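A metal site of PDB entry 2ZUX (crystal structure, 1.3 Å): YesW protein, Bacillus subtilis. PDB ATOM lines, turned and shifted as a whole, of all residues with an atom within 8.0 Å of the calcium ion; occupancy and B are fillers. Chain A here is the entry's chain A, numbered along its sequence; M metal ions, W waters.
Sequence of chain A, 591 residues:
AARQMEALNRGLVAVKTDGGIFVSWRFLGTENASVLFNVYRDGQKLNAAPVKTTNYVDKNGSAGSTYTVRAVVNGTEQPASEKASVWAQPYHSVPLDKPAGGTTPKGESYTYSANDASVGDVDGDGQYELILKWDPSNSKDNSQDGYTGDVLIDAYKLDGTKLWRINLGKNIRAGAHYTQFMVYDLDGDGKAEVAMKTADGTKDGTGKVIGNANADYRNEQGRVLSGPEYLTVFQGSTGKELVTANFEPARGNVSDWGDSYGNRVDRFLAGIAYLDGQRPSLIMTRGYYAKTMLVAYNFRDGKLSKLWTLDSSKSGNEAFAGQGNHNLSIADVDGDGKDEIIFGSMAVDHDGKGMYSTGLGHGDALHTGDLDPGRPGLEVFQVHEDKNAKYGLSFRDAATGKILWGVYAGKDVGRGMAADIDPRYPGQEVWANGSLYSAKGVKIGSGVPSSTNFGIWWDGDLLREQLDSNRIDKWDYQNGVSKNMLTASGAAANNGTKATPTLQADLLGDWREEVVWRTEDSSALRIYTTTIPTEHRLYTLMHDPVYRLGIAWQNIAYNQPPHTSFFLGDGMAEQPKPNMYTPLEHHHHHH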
ATOM      1  N   GLY A  11       3.376   4.531  24.172  1.00  0.00           N
ATOM      2  CA  GLY A  11       4.814   4.568  23.878  1.00  0.00           C
ATOM      3  C   GLY A  11       5.638   3.928  24.975  1.00  0.00           C
ATOM      4  O   GLY A  11       6.801   4.270  25.170  1.00  0.00           O
ATOM      5  N   VAL A  13       8.047   1.812  27.101  1.00  0.00           N
ATOM      6  CA  VAL A  13       9.307   1.110  26.837  1.00  0.00           C
ATOM      7  C   VAL A  13       9.935   0.691  28.163  1.00  0.00           C
ATOM      8  O   VAL A  13       9.802   1.401  29.174  1.00  0.00           O
ATOM      9  CB  VAL A  13      10.277   2.002  25.981  1.00  0.00           C
ATOM     10  CG1 VAL A  13      10.865   3.145  26.789  1.00  0.00           C
ATOM     11  CG2 VAL A  13      11.393   1.164  25.363  1.00  0.00           C
ATOM     12  N   SER A  24       9.836   3.972  30.725  1.00  0.00           N
ATOM     13  CA  SER A  24       9.347   5.320  30.419  1.00  0.00           C
ATOM     14  C   SER A  24       8.215   5.269  29.406  1.00  0.00           C
ATOM     15  O   SER A  24       8.028   4.281  28.689  1.00  0.00           O
ATOM     16  CB  SER A  24      10.467   6.307  30.031  1.00  0.00           C
ATOM     17  OG  SER A  24      10.801   6.236  28.644  1.00  0.00           O
ATOM     18  N   TRP A  25       7.420   6.340  29.396  1.00  0.00           N
ATOM     19  CA  TRP A  25       6.220   6.371  28.583  1.00  0.00           C
ATOM     20  C   TRP A  25       5.820   7.814  28.288  1.00  0.00           C
ATOM     21  O   TRP A  25       6.388   8.760  28.842  1.00  0.00           O
ATOM     22  CB  TRP A  25       5.068   5.605  29.255  1.00  0.00           C
ATOM     23  CG  TRP A  25       4.634   6.147  30.588  1.00  0.00           C
ATOM     24  CD1 TRP A  25       3.638   7.055  30.828  1.00  0.00           C
ATOM     25  CD2 TRP A  25       5.199   5.833  31.877  1.00  0.00           C
ATOM     26  NE1 TRP A  25       3.535   7.308  32.184  1.00  0.00           N
ATOM     27  CE2 TRP A  25       4.478   6.564  32.850  1.00  0.00           C
ATOM     28  CE3 TRP A  25       6.234   4.992  32.297  1.00  0.00           C
ATOM     29  CZ2 TRP A  25       4.770   6.499  34.216  1.00  0.00           C
ATOM     30  CZ3 TRP A  25       6.519   4.915  33.666  1.00  0.00           C
ATOM     31  CH2 TRP A  25       5.795   5.665  34.607  1.00  0.00           C
ATOM     32  N   ARG A  26       4.835   7.970  27.411  1.00  0.00           N
ATOM     33  CA  ARG A  26       4.397   9.291  26.963  1.00  0.00           C
ATOM     34  C   ARG A  26       3.417   9.938  27.902  1.00  0.00           C
ATOM     35  O   ARG A  26       2.539   9.274  28.474  1.00  0.00           O
ATOM     36  CB  ARG A  26       3.718   9.177  25.604  1.00  0.00           C
ATOM     37  CG  ARG A  26       4.617   8.725  24.480  1.00  0.00           C
ATOM     38  CD  ARG A  26       3.794   8.369  23.267  1.00  0.00           C
ATOM     39  NE  ARG A  26       4.630   8.160  22.101  1.00  0.00           N
ATOM     40  CZ  ARG A  26       4.355   7.318  21.108  1.00  0.00           C
ATOM     41  NH1 ARG A  26       3.280   6.532  21.130  1.00  0.00           N
ATOM     42  NH2 ARG A  26       5.189   7.239  20.078  1.00  0.00           N
ATOM     43  N   TRP A 457      17.810  16.221  23.522  1.00  0.00           N
ATOM     44  CA  TRP A 457      17.454  16.050  24.938  1.00  0.00           C
ATOM     45  C   TRP A 457      17.655  14.597  25.304  1.00  0.00           C
ATOM     46  O   TRP A 457      16.885  13.739  24.888  1.00  0.00           O
ATOM     47  CB  TRP A 457      16.014  16.508  25.222  1.00  0.00           C
ATOM     48  CG  TRP A 457      15.868  18.001  25.085  1.00  0.00           C
ATOM     49  CD1 TRP A 457      16.439  18.950  25.900  1.00  0.00           C
ATOM     50  CD2 TRP A 457      15.135  18.714  24.083  1.00  0.00           C
ATOM     51  NE1 TRP A 457      16.108  20.215  25.451  1.00  0.00           N
ATOM     52  CE2 TRP A 457      15.320  20.100  24.337  1.00  0.00           C
ATOM     53  CE3 TRP A 457      14.360  18.325  22.979  1.00  0.00           C
ATOM     54  CZ2 TRP A 457      14.736  21.084  23.542  1.00  0.00           C
ATOM     55  CZ3 TRP A 457      13.775  19.319  22.187  1.00  0.00           C
ATOM     56  CH2 TRP A 457      13.986  20.681  22.468  1.00  0.00           C
ATOM     57  N   TRP A 458      18.723  14.330  26.064  1.00  0.00           N
ATOM     58  CA  TRP A 458      19.131  12.949  26.363  1.00  0.00           C
ATOM     59  C   TRP A 458      19.179  12.606  27.841  1.00  0.00           C
ATOM     60  O   TRP A 458      18.712  11.533  28.234  1.00  0.00           O
ATOM     61  CB  TRP A 458      20.494  12.660  25.723  1.00  0.00           C
ATOM     62  CG  TRP A 458      20.931  11.249  25.921  1.00  0.00           C
ATOM     63  CD1 TRP A 458      21.927  10.806  26.744  1.00  0.00           C
ATOM     64  CD2 TRP A 458      20.385  10.086  25.292  1.00  0.00           C
ATOM     65  NE1 TRP A 458      22.045   9.436  26.645  1.00  0.00           N
ATOM     66  CE2 TRP A 458      21.100   8.969  25.768  1.00  0.00           C
ATOM     67  CE3 TRP A 458      19.359   9.875  24.351  1.00  0.00           C
ATOM     68  CZ2 TRP A 458      20.831   7.659  25.338  1.00  0.00           C
ATOM     69  CZ3 TRP A 458      19.094   8.573  23.932  1.00  0.00           C
ATOM     70  CH2 TRP A 458      19.828   7.493  24.437  1.00  0.00           C
ATOM     71  N   ALA A 505      14.488  11.575  17.199  1.00  0.00           N
ATOM     72  CA  ALA A 505      13.096  11.963  17.462  1.00  0.00           C
ATOM     73  C   ALA A 505      12.652  11.339  18.760  1.00  0.00           C
ATOM     74  O   ALA A 505      13.055  10.212  19.090  1.00  0.00           O
ATOM     75  CB  ALA A 505      12.182  11.496  16.336  1.00  0.00           C
ATOM     76  N   ASP A 506      11.780  12.032  19.476  1.00  0.00           N
ATOM     77  CA  ASP A 506      11.061  11.393  20.587  1.00  0.00           C
ATOM     78  C   ASP A 506       9.994  10.467  20.016  1.00  0.00           C
ATOM     79  O   ASP A 506       8.850  10.871  19.785  1.00  0.00           O
ATOM     80  CB  ASP A 506      10.404  12.435  21.498  1.00  0.00           C
ATOM     81  CG  ASP A 506       9.561  11.796  22.575  1.00  0.00           C
ATOM     82  OD1 ASP A 506       9.777  10.610  22.896  1.00  0.00           O
ATOM     83  OD2 ASP A 506       8.679  12.499  23.098  1.00  0.00           O
ATOM     84  N   LEU A 507      10.387   9.212  19.770  1.00  0.00           N
ATOM     85  CA  LEU A 507       9.478   8.276  19.131  1.00  0.00           C
ATOM     86  C   LEU A 507       8.890   7.217  20.055  1.00  0.00           C
ATOM     87  O   LEU A 507       7.968   6.516  19.663  1.00  0.00           O
ATOM     88  CB  LEU A 507      10.089   7.649  17.867  1.00  0.00           C
ATOM     89  CG  LEU A 507      11.525   7.144  17.829  1.00  0.00           C
ATOM     90  CD1 LEU A 507      11.684   5.871  18.630  1.00  0.00           C
ATOM     91  CD2 LEU A 507      11.967   6.906  16.386  1.00  0.00           C
ATOM     92  N   LEU A 508       9.425   7.097  21.270  1.00  0.00           N
ATOM     93  CA  LEU A 508       8.858   6.213  22.293  1.00  0.00           C
ATOM     94  C   LEU A 508       9.274   6.712  23.667  1.00  0.00           C
ATOM     95  O   LEU A 508      10.128   7.585  23.771  1.00  0.00           O
ATOM     96  CB  LEU A 508       9.251   4.748  22.088  1.00  0.00           C
ATOM     97  CG  LEU A 508      10.709   4.387  21.843  1.00  0.00           C
ATOM     98  CD1 LEU A 508      11.492   4.303  23.143  1.00  0.00           C
ATOM     99  CD2 LEU A 508      10.791   3.054  21.086  1.00  0.00           C
ATOM    100  N   GLY A 509       8.648   6.189  24.714  1.00  0.00           N
ATOM    101  CA  GLY A 509       9.018   6.561  26.065  1.00  0.00           C
ATOM    102  C   GLY A 509       8.656   7.998  26.393  1.00  0.00           C
ATOM    103  O   GLY A 509       7.773   8.583  25.770  1.00  0.00           O
ATOM    104  N   ASP A 510       9.368   8.555  27.381  1.00  0.00           N
ATOM    105  CA  ASP A 510       9.116   9.926  27.818  1.00  0.00           C
ATOM    106  C   ASP A 510       9.738  10.951  26.889  1.00  0.00           C
ATOM    107  O   ASP A 510      10.219  10.621  25.805  1.00  0.00           O
ATOM    108  CB  ASP A 510       9.525  10.121  29.301  1.00  0.00           C
ATOM    109  CG  ASP A 510      11.038  10.124  29.522  1.00  0.00           C
ATOM    110  OD1 ASP A 510      11.829  10.262  28.557  1.00  0.00           O
ATOM    111  OD2 ASP A 510      11.438  10.043  30.706  1.00  0.00           O
ATOM    112  N   TRP A 511       9.744  12.205  27.330  1.00  0.00           N
ATOM    113  CA  TRP A 511      10.049  13.333  26.451  1.00  0.00           C
ATOM    114  C   TRP A 511      11.459  13.382  25.866  1.00  0.00           C
ATOM    115  O   TRP A 511      11.684  14.119  24.911  1.00  0.00           O
ATOM    116  CB  TRP A 511       9.744  14.651  27.169  1.00  0.00           C
ATOM    117  CG  TRP A 511      10.602  14.911  28.367  1.00  0.00           C
ATOM    118  CD1 TRP A 511      10.391  14.445  29.643  1.00  0.00           C
ATOM    119  CD2 TRP A 511      11.798  15.703  28.433  1.00  0.00           C
ATOM    120  NE1 TRP A 511      11.390  14.891  30.477  1.00  0.00           N
ATOM    121  CE2 TRP A 511      12.269  15.658  29.757  1.00  0.00           C
ATOM    122  CE3 TRP A 511      12.529  16.437  27.479  1.00  0.00           C
ATOM    123  CZ2 TRP A 511      13.419  16.335  30.176  1.00  0.00           C
ATOM    124  CZ3 TRP A 511      13.679  17.114  27.898  1.00  0.00           C
ATOM    125  CH2 TRP A 511      14.108  17.051  29.226  1.00  0.00           C
ATOM    126  N   ARG A 512      12.398  12.605  26.417  1.00  0.00           N
ATOM    127  CA  ARG A 512      13.732  12.621  25.833  1.00  0.00           C
ATOM    128  C   ARG A 512      13.702  12.026  24.422  1.00  0.00           C
ATOM    129  O   ARG A 512      12.816  11.244  24.079  1.00  0.00           O
ATOM    130  CB  ARG A 512      14.753  11.912  26.722  1.00  0.00           C
ATOM    131  CG  ARG A 512      15.360  12.801  27.816  1.00  0.00           C
ATOM    132  CD  ARG A 512      14.409  13.040  28.996  1.00  0.00           C
ATOM    133  NE  ARG A 512      14.000  11.814  29.673  1.00  0.00           N
ATOM    134  CZ  ARG A 512      14.734  11.155  30.557  1.00  0.00           C
ATOM    135  NH1 ARG A 512      14.255  10.045  31.116  1.00  0.00           N
ATOM    136  NH2 ARG A 512      15.951  11.574  30.887  1.00  0.00           N
ATOM    137  N   GLU A 513      14.669  12.438  23.594  1.00  0.00           N
ATOM    138  CA  GLU A 513      14.701  12.013  22.213  1.00  0.00           C
ATOM    139  C   GLU A 513      15.462  10.704  22.036  1.00  0.00           C
ATOM    140  O   GLU A 513      16.505  10.500  22.624  1.00  0.00           O
ATOM    141  CB  GLU A 513      15.334  13.108  21.374  1.00  0.00           C
ATOM    142  CG  GLU A 513      14.592  14.430  21.477  1.00  0.00           C
ATOM    143  CD  GLU A 513      15.244  15.522  20.662  1.00  0.00           C
ATOM    144  OE1 GLU A 513      16.120  16.222  21.225  1.00  0.00           O
ATOM    145  OE2 GLU A 513      14.907  15.649  19.464  1.00  0.00           O
ATOM    146  N   GLU A 514      14.909   9.815  21.204  1.00  0.00           N
ATOM    147  CA  GLU A 514      15.588   8.586  20.799  1.00  0.00           C
ATOM    148  C   GLU A 514      16.506   8.895  19.628  1.00  0.00           C
ATOM    149  O   GLU A 514      16.330   9.899  18.924  1.00  0.00           O
ATOM    150  CB  GLU A 514      14.588   7.522  20.385  1.00  0.00           C
ATOM    151  CG  GLU A 514      13.844   6.849  21.533  1.00  0.00           C
ATOM    152  CD  GLU A 514      13.038   7.817  22.393  1.00  0.00           C
ATOM    153  OE1 GLU A 514      12.162   8.539  21.849  1.00  0.00           O
ATOM    154  OE2 GLU A 514      13.284   7.867  23.622  1.00  0.00           O
ATOM    155  N   VAL A 515      17.509   8.036  19.442  1.00  0.00           N
ATOM    156  CA  VAL A 515      18.372   8.115  18.276  1.00  0.00           C
ATOM    157  C   VAL A 515      18.306   6.811  17.521  1.00  0.00           C
ATOM    158  O   VAL A 515      18.388   5.726  18.120  1.00  0.00           O
ATOM    159  CB  VAL A 515      19.838   8.386  18.637  1.00  0.00           C
ATOM    160  CG1 VAL A 515      20.634   8.699  17.382  1.00  0.00           C
ATOM    161  CG2 VAL A 515      19.953   9.508  19.629  1.00  0.00           C
ATOM    162  N   TYR A 528      18.180   3.815  20.122  1.00  0.00           N
ATOM    163  CA  TYR A 528      18.639   4.070  21.490  1.00  0.00           C
ATOM    164  C   TYR A 528      17.630   4.964  22.199  1.00  0.00           C
ATOM    165  O   TYR A 528      17.215   5.981  21.649  1.00  0.00           O
ATOM    166  CB  TYR A 528      19.998   4.765  21.468  1.00  0.00           C
ATOM    167  CG  TYR A 528      21.151   3.884  21.030  1.00  0.00           C
ATOM    168  CD1 TYR A 528      22.060   3.383  21.972  1.00  0.00           C
ATOM    169  CD2 TYR A 528      21.339   3.543  19.697  1.00  0.00           C
ATOM    170  CE1 TYR A 528      23.118   2.569  21.577  1.00  0.00           C
ATOM    171  CE2 TYR A 528      22.405   2.732  19.296  1.00  0.00           C
ATOM    172  CZ  TYR A 528      23.281   2.257  20.241  1.00  0.00           C
ATOM    173  OH  TYR A 528      24.328   1.446  19.830  1.00  0.00           O
ATOM    174  N   THR A 529      17.230   4.562  23.399  1.00  0.00           N
ATOM    175  CA  THR A 529      16.371   5.377  24.249  1.00  0.00           C
ATOM    176  C   THR A 529      17.112   5.588  25.564  1.00  0.00           C
ATOM    177  O   THR A 529      17.803   4.687  26.041  1.00  0.00           O
ATOM    178  CB  THR A 529      14.970   4.740  24.460  1.00  0.00           C
ATOM    179  OG1 THR A 529      14.068   5.713  25.016  1.00  0.00           O
ATOM    180  CG2 THR A 529      15.013   3.517  25.393  1.00  0.00           C
ATOM    181  N   THR A 530      16.982   6.769  26.156  1.00  0.00           N
ATOM    182  CA  THR A 530      17.710   7.054  27.379  1.00  0.00           C
ATOM    183  C   THR A 530      17.192   6.239  28.564  1.00  0.00           C
ATOM    184  O   THR A 530      15.991   5.945  28.669  1.00  0.00           O
ATOM    185  CB  THR A 530      17.711   8.561  27.700  1.00  0.00           C
ATOM    186  OG1 THR A 530      18.700   8.813  28.699  1.00  0.00           O
ATOM    187  CG2 THR A 530      16.356   9.044  28.213  1.00  0.00           C
ATOM    188  N   THR A 540       4.704  14.523  25.076  1.00  0.00           N
ATOM    189  CA  THR A 540       5.505  13.920  24.026  1.00  0.00           C
ATOM    190  C   THR A 540       5.792  14.953  22.945  1.00  0.00           C
ATOM    191  O   THR A 540       4.912  15.728  22.551  1.00  0.00           O
ATOM    192  CB  THR A 540       4.855  12.643  23.444  1.00  0.00           C
ATOM    193  OG1 THR A 540       5.708  12.116  22.417  1.00  0.00           O
ATOM    194  CG2 THR A 540       3.475  12.913  22.840  1.00  0.00           C
ATOM    195  N   LEU A 541       7.041  15.004  22.492  1.00  0.00           N
ATOM    196  CA  LEU A 541       7.451  16.071  21.589  1.00  0.00           C
ATOM    197  C   LEU A 541       6.762  15.986  20.230  1.00  0.00           C
ATOM    198  O   LEU A 541       6.611  16.988  19.544  1.00  0.00           O
ATOM    199  CB  LEU A 541       8.976  16.099  21.455  1.00  0.00           C
ATOM    200  CG  LEU A 541       9.770  16.174  22.759  1.00  0.00           C
ATOM    201  CD1 LEU A 541      11.259  16.282  22.464  1.00  0.00           C
ATOM    202  CD2 LEU A 541       9.292  17.345  23.646  1.00  0.00           C
ATOM    203  N   TYR A 547       7.947  20.829  16.668  1.00  0.00           N
ATOM    204  CA  TYR A 547       8.797  19.664  16.748  1.00  0.00           C
ATOM    205  C   TYR A 547       8.344  18.581  15.762  1.00  0.00           C
ATOM    206  O   TYR A 547       9.153  18.003  15.049  1.00  0.00           O
ATOM    207  CB  TYR A 547       8.835  19.112  18.177  1.00  0.00           C
ATOM    208  CG  TYR A 547       9.833  17.992  18.367  1.00  0.00           C
ATOM    209  CD1 TYR A 547      11.093  18.242  18.878  1.00  0.00           C
ATOM    210  CD2 TYR A 547       9.496  16.689  18.026  1.00  0.00           C
ATOM    211  CE1 TYR A 547      12.023  17.202  19.044  1.00  0.00           C
ATOM    212  CE2 TYR A 547      10.398  15.645  18.188  1.00  0.00           C
ATOM    213  CZ  TYR A 547      11.641  15.913  18.700  1.00  0.00           C
ATOM    214  OH  TYR A 547      12.511  14.859  18.846  1.00  0.00           O
HETATM  215 CA    CA M   1      11.428   9.421  24.185  1.00  0.00          CA
HETATM  216  O   HOH W   1      12.378   8.814  26.346  1.00  0.00           O
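The calcium ion is bound by O of Leu 508 (2.3 Å), O of Arg 512 (2.3 Å), O of Asp 510 (2.4 Å), OD1 of Asp 506 (2.4 Å), water W1 (2.4 Å), OE2 of Glu 514 (2.5 Å) and OE1 of Glu 514 (2.6 Å).
Residues that only touch the calcium ion: Gly 509 (3.8 Å).
OD2 of Asp 506 is in hydrogen-bond range of OG1 of Thr 540, at 3.1 Å. N of Leu 541 sits at hydrogen-bond distance from OD2 of Asp 506 (3.1 Å). The backbone NH of Asp 506 sits at hydrogen-bond distance from the side-chain hydroxyl of Tyr 547, at 3.0 Å. The guanidinium group (NH1) of Arg 512 is in salt-bridge range of the side-chain carboxylate (OD2) of Asp 510 (2.8 Å). The backbone NH (N) of Asp 510 sits close to the backbone carbonyl oxygen (O) of Trp 25. The backbone NH of Glu 514 sits at hydrogen-bond distance from the backbone carbonyl oxygen of Ala 505, at 2.8 Å. The backbone NH of Asp 510 sits at hydrogen-bond distance from the side-chain hydroxyl of Ser 24 (3.0 Å). N of Gly 509 is in hydrogen-bond range of O of Gly 11, 2.7 Å away.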
